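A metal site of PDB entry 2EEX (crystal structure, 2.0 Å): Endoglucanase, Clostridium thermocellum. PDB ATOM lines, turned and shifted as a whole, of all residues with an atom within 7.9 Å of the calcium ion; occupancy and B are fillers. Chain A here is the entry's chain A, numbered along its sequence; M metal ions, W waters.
The backbone carbonyl oxygen (O) of Asp 153 is in hydrogen-bond range of the side-chain amino group (NZ) of Lys 135, at 2.8 Å.
The backbone NH (N) of Glu 54 is in hydrogen-bond range of the side-chain amide oxygen (OD1) of Asn 52, 2.9 Å away.
The side-chain carboxylate of Asp 150 sits at hydrogen-bond distance from the backbone NH of Glu 152 (2.6 Å).
The nearest printed residue that does not touch the calcium ion is Thr 151 (4.3 Å).
The calcium ion is bound by O of Tyr 155 (2.2 Å), O of Asp 150 (2.3 Å), water W1 (2.4 Å), OD1 of Asp 153 (2.4 Å), OE2 of Glu 54 (2.4 Å), OE1 of Glu 54 (2.5 Å) and water W2 (2.5 Å).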
ATOM      1  N   ASN A  52      15.426  -7.777  -7.886  1.00  0.00           N
ATOM      2  CA  ASN A  52      16.222  -8.647  -8.755  1.00  0.00           C
ATOM      3  C   ASN A  52      17.510  -7.929  -9.126  1.00  0.00           C
ATOM      4  O   ASN A  52      17.489  -7.016  -9.953  1.00  0.00           O
ATOM      5  CB  ASN A  52      15.437  -8.987 -10.017  1.00  0.00           C
ATOM      6  CG  ASN A  52      16.144 -10.018 -10.891  1.00  0.00           C
ATOM      7  OD1 ASN A  52      17.365 -10.140 -10.845  1.00  0.00           O
ATOM      8  ND2 ASN A  52      15.364 -10.749 -11.693  1.00  0.00           N
ATOM      9  N   TRP A  53      18.631  -8.339  -8.542  1.00  0.00           N
ATOM     10  CA  TRP A  53      19.901  -7.692  -8.835  1.00  0.00           C
ATOM     11  C   TRP A  53      20.348  -7.782 -10.292  1.00  0.00           C
ATOM     12  O   TRP A  53      21.102  -6.933 -10.775  1.00  0.00           O
ATOM     13  CB  TRP A  53      21.007  -8.258  -7.932  1.00  0.00           C
ATOM     14  CG  TRP A  53      21.593  -9.561  -8.382  1.00  0.00           C
ATOM     15  CD1 TRP A  53      21.050 -10.812  -8.232  1.00  0.00           C
ATOM     16  CD2 TRP A  53      22.851  -9.756  -9.037  1.00  0.00           C
ATOM     17  NE1 TRP A  53      21.894 -11.769  -8.761  1.00  0.00           N
ATOM     18  CE2 TRP A  53      23.005 -11.136  -9.263  1.00  0.00           C
ATOM     19  CE3 TRP A  53      23.868  -8.881  -9.458  1.00  0.00           C
ATOM     20  CZ2 TRP A  53      24.140 -11.672  -9.890  1.00  0.00           C
ATOM     21  CZ3 TRP A  53      25.000  -9.408 -10.084  1.00  0.00           C
ATOM     22  CH2 TRP A  53      25.118 -10.797 -10.290  1.00  0.00           C
ATOM     23  N   GLU A  54      19.888  -8.804 -11.000  1.00  0.00           N
ATOM     24  CA  GLU A  54      20.270  -8.992 -12.398  1.00  0.00           C
ATOM     25  C   GLU A  54      19.758  -7.879 -13.304  1.00  0.00           C
ATOM     26  O   GLU A  54      20.426  -7.508 -14.276  1.00  0.00           O
ATOM     27  CB  GLU A  54      19.779 -10.338 -12.923  1.00  0.00           C
ATOM     28  CG  GLU A  54      20.196 -11.564 -12.100  1.00  0.00           C
ATOM     29  CD  GLU A  54      19.903 -12.871 -12.801  1.00  0.00           C
ATOM     30  OE1 GLU A  54      18.991 -12.901 -13.649  1.00  0.00           O
ATOM     31  OE2 GLU A  54      20.576 -13.884 -12.519  1.00  0.00           O
ATOM     32  N   ASN A  55      18.582  -7.335 -12.996  1.00  0.00           N
ATOM     33  CA  ASN A  55      18.010  -6.266 -13.823  1.00  0.00           C
ATOM     34  C   ASN A  55      17.484  -5.069 -13.028  1.00  0.00           C
ATOM     35  O   ASN A  55      16.968  -4.117 -13.621  1.00  0.00           O
ATOM     36  CB  ASN A  55      16.888  -6.845 -14.693  1.00  0.00           C
ATOM     37  CG  ASN A  55      15.855  -7.603 -13.879  1.00  0.00           C
ATOM     38  OD1 ASN A  55      15.541  -7.235 -12.749  1.00  0.00           O
ATOM     39  ND2 ASN A  55      15.316  -8.668 -14.452  1.00  0.00           N
ATOM     40  N   LYS A 135      11.211 -14.723 -11.066  1.00  0.00           N
ATOM     41  CA  LYS A 135      12.391 -15.551 -11.246  1.00  0.00           C
ATOM     42  C   LYS A 135      12.591 -16.181  -9.873  1.00  0.00           C
ATOM     43  O   LYS A 135      12.479 -15.496  -8.860  1.00  0.00           O
ATOM     44  CB  LYS A 135      13.618 -14.718 -11.609  1.00  0.00           C
ATOM     45  CG  LYS A 135      13.557 -14.060 -12.978  1.00  0.00           C
ATOM     46  CD  LYS A 135      13.451 -15.089 -14.094  1.00  0.00           C
ATOM     47  CE  LYS A 135      13.444 -14.408 -15.458  1.00  0.00           C
ATOM     48  NZ  LYS A 135      13.233 -15.389 -16.552  1.00  0.00           N
ATOM     49  N   GLU A 136      12.867 -17.475  -9.837  1.00  0.00           N
ATOM     50  CA  GLU A 136      13.091 -18.169  -8.579  1.00  0.00           C
ATOM     51  C   GLU A 136      14.469 -17.862  -8.035  1.00  0.00           C
ATOM     52  O   GLU A 136      15.458 -17.859  -8.765  1.00  0.00           O
ATOM     53  CB  GLU A 136      12.963 -19.685  -8.763  1.00  0.00           C
ATOM     54  CG  GLU A 136      13.052 -20.460  -7.464  1.00  0.00           C
ATOM     55  CD  GLU A 136      12.986 -21.963  -7.682  1.00  0.00           C
ATOM     56  OE1 GLU A 136      12.214 -22.404  -8.562  1.00  0.00           O
ATOM     57  OE2 GLU A 136      13.690 -22.701  -6.967  1.00  0.00           O
ATOM     58  N   LYS A 141      24.596 -20.833  -6.467  1.00  0.00           N
ATOM     59  CA  LYS A 141      24.560 -21.137  -7.885  1.00  0.00           C
ATOM     60  C   LYS A 141      25.011 -22.569  -8.180  1.00  0.00           C
ATOM     61  O   LYS A 141      24.421 -23.263  -9.018  1.00  0.00           O
ATOM     62  CB  LYS A 141      25.433 -20.144  -8.675  1.00  0.00           C
ATOM     63  CG  LYS A 141      25.310 -20.298 -10.187  1.00  0.00           C
ATOM     64  CD  LYS A 141      26.047 -19.198 -10.927  1.00  0.00           C
ATOM     65  CE  LYS A 141      25.815 -19.304 -12.426  1.00  0.00           C
ATOM     66  NZ  LYS A 141      26.596 -18.280 -13.189  1.00  0.00           N
ATOM     67  N   PRO A 149      25.363 -11.768 -15.124  1.00  0.00           N
ATOM     68  CA  PRO A 149      24.319 -12.777 -14.912  1.00  0.00           C
ATOM     69  C   PRO A 149      23.347 -12.943 -16.077  1.00  0.00           C
ATOM     70  O   PRO A 149      23.030 -11.986 -16.790  1.00  0.00           O
ATOM     71  CB  PRO A 149      23.621 -12.299 -13.645  1.00  0.00           C
ATOM     72  CG  PRO A 149      23.776 -10.804 -13.715  1.00  0.00           C
ATOM     73  CD  PRO A 149      25.215 -10.663 -14.156  1.00  0.00           C
ATOM     74  N   ASP A 150      22.895 -14.176 -16.274  1.00  0.00           N
ATOM     75  CA  ASP A 150      21.958 -14.518 -17.328  1.00  0.00           C
ATOM     76  C   ASP A 150      20.558 -14.091 -16.897  1.00  0.00           C
ATOM     77  O   ASP A 150      20.005 -14.641 -15.949  1.00  0.00           O
ATOM     78  CB  ASP A 150      21.980 -16.020 -17.571  1.00  0.00           C
ATOM     79  CG  ASP A 150      21.217 -16.432 -18.821  1.00  0.00           C
ATOM     80  OD1 ASP A 150      20.234 -15.753 -19.178  1.00  0.00           O
ATOM     81  OD2 ASP A 150      21.596 -17.457 -19.427  1.00  0.00           O
ATOM     82  N   THR A 151      19.977 -13.123 -17.592  1.00  0.00           N
ATOM     83  CA  THR A 151      18.644 -12.634 -17.255  1.00  0.00           C
ATOM     84  C   THR A 151      17.580 -13.456 -17.969  1.00  0.00           C
ATOM     85  O   THR A 151      16.378 -13.236 -17.766  1.00  0.00           O
ATOM     86  CB  THR A 151      18.464 -11.166 -17.677  1.00  0.00           C
ATOM     87  OG1 THR A 151      18.625 -11.057 -19.097  1.00  0.00           O
ATOM     88  CG2 THR A 151      19.497 -10.287 -16.980  1.00  0.00           C
ATOM     89  N   GLU A 152      18.008 -14.399 -18.796  1.00  0.00           N
ATOM     90  CA  GLU A 152      17.092 -15.221 -19.568  1.00  0.00           C
ATOM     91  C   GLU A 152      16.667 -16.525 -18.890  1.00  0.00           C
ATOM     92  O   GLU A 152      15.600 -17.058 -19.199  1.00  0.00           O
ATOM     93  CB  GLU A 152      17.686 -15.532 -20.942  1.00  0.00           C
ATOM     94  CG  GLU A 152      18.142 -14.287 -21.693  1.00  0.00           C
ATOM     95  CD  GLU A 152      17.054 -13.234 -21.784  1.00  0.00           C
ATOM     96  OE1 GLU A 152      16.019 -13.486 -22.435  1.00  0.00           O
ATOM     97  OE2 GLU A 152      17.234 -12.145 -21.187  1.00  0.00           O
ATOM     98  N   ASP A 153      17.497 -17.067 -17.998  1.00  0.00           N
ATOM     99  CA  ASP A 153      17.119 -18.299 -17.346  1.00  0.00           C
ATOM    100  C   ASP A 153      16.055 -18.006 -16.287  1.00  0.00           C
ATOM    101  O   ASP A 153      15.588 -16.877 -16.171  1.00  0.00           O
ATOM    102  CB  ASP A 153      18.335 -19.020 -16.728  1.00  0.00           C
ATOM    103  CG  ASP A 153      19.072 -18.175 -15.723  1.00  0.00           C
ATOM    104  OD1 ASP A 153      18.466 -17.290 -15.094  1.00  0.00           O
ATOM    105  OD2 ASP A 153      20.288 -18.429 -15.546  1.00  0.00           O
ATOM    106  N   ASP A 154      15.664 -19.013 -15.519  1.00  0.00           N
ATOM    107  CA  ASP A 154      14.612 -18.824 -14.521  1.00  0.00           C
ATOM    108  C   ASP A 154      15.065 -18.619 -13.075  1.00  0.00           C
ATOM    109  O   ASP A 154      14.242 -18.644 -12.162  1.00  0.00           O
ATOM    110  CB  ASP A 154      13.658 -20.019 -14.548  1.00  0.00           C
ATOM    111  CG  ASP A 154      12.983 -20.189 -15.896  1.00  0.00           C
ATOM    112  OD1 ASP A 154      12.432 -19.192 -16.414  1.00  0.00           O
ATOM    113  OD2 ASP A 154      13.005 -21.316 -16.420  1.00  0.00           O
ATOM    114  N   TYR A 155      16.356 -18.375 -12.870  1.00  0.00           N
ATOM    115  CA  TYR A 155      16.891 -18.211 -11.525  1.00  0.00           C
ATOM    116  C   TYR A 155      17.760 -16.991 -11.282  1.00  0.00           C
ATOM    117  O   TYR A 155      18.382 -16.463 -12.199  1.00  0.00           O
ATOM    118  CB  TYR A 155      17.719 -19.441 -11.164  1.00  0.00           C
ATOM    119  CG  TYR A 155      16.972 -20.747 -11.278  1.00  0.00           C
ATOM    120  CD1 TYR A 155      16.136 -21.181 -10.258  1.00  0.00           C
ATOM    121  CD2 TYR A 155      17.101 -21.555 -12.412  1.00  0.00           C
ATOM    122  CE1 TYR A 155      15.439 -22.379 -10.356  1.00  0.00           C
ATOM    123  CE2 TYR A 155      16.410 -22.757 -12.525  1.00  0.00           C
ATOM    124  CZ  TYR A 155      15.575 -23.161 -11.495  1.00  0.00           C
ATOM    125  OH  TYR A 155      14.891 -24.345 -11.577  1.00  0.00           O
ATOM    126  N   VAL A 156      17.791 -16.564 -10.022  1.00  0.00           N
ATOM    127  CA  VAL A 156      18.613 -15.440  -9.592  1.00  0.00           C
ATOM    128  C   VAL A 156      19.378 -15.983  -8.380  1.00  0.00           C
ATOM    129  O   VAL A 156      18.767 -16.470  -7.424  1.00  0.00           O
ATOM    130  CB  VAL A 156      17.771 -14.221  -9.183  1.00  0.00           C
ATOM    131  CG1 VAL A 156      18.665 -13.139  -8.621  1.00  0.00           C
ATOM    132  CG2 VAL A 156      17.014 -13.674 -10.400  1.00  0.00           C
ATOM    133  N   TYR A 157      20.700 -15.904  -8.427  1.00  0.00           N
ATOM    134  CA  TYR A 157      21.532 -16.452  -7.353  1.00  0.00           C
ATOM    135  C   TYR A 157      22.073 -15.421  -6.371  1.00  0.00           C
ATOM    136  O   TYR A 157      22.712 -14.445  -6.749  1.00  0.00           O
ATOM    137  CB  TYR A 157      22.678 -17.229  -7.981  1.00  0.00           C
ATOM    138  CG  TYR A 157      22.181 -18.295  -8.919  1.00  0.00           C
ATOM    139  CD1 TYR A 157      21.658 -19.487  -8.440  1.00  0.00           C
ATOM    140  CD2 TYR A 157      22.201 -18.102 -10.299  1.00  0.00           C
ATOM    141  CE1 TYR A 157      21.154 -20.462  -9.296  1.00  0.00           C
ATOM    142  CE2 TYR A 157      21.699 -19.059 -11.179  1.00  0.00           C
ATOM    143  CZ  TYR A 157      21.180 -20.237 -10.657  1.00  0.00           C
ATOM    144  OH  TYR A 157      20.696 -21.203 -11.512  1.00  0.00           O
ATOM    145  N   GLU A 160      25.949 -15.292  -6.165  1.00  0.00           N
ATOM    146  CA  GLU A 160      26.532 -14.683  -7.370  1.00  0.00           C
ATOM    147  C   GLU A 160      26.425 -13.165  -7.218  1.00  0.00           C
ATOM    148  O   GLU A 160      27.300 -12.412  -7.628  1.00  0.00           O
ATOM    149  CB  GLU A 160      25.788 -15.139  -8.630  1.00  0.00           C
ATOM    150  CG  GLU A 160      26.369 -14.590  -9.923  1.00  0.00           C
ATOM    151  CD  GLU A 160      25.818 -15.290 -11.157  1.00  0.00           C
ATOM    152  OE1 GLU A 160      24.582 -15.273 -11.363  1.00  0.00           O
ATOM    153  OE2 GLU A 160      26.624 -15.853 -11.923  1.00  0.00           O
HETATM  154 CA    CA M   1      19.259 -15.345 -13.937  1.00  0.00          CA
HETATM  155  O   HOH W   1      21.207 -16.678 -13.669  1.00  0.00           O
HETATM  156  O   HOH W   2      16.924 -14.859 -14.604  1.00  0.00           O
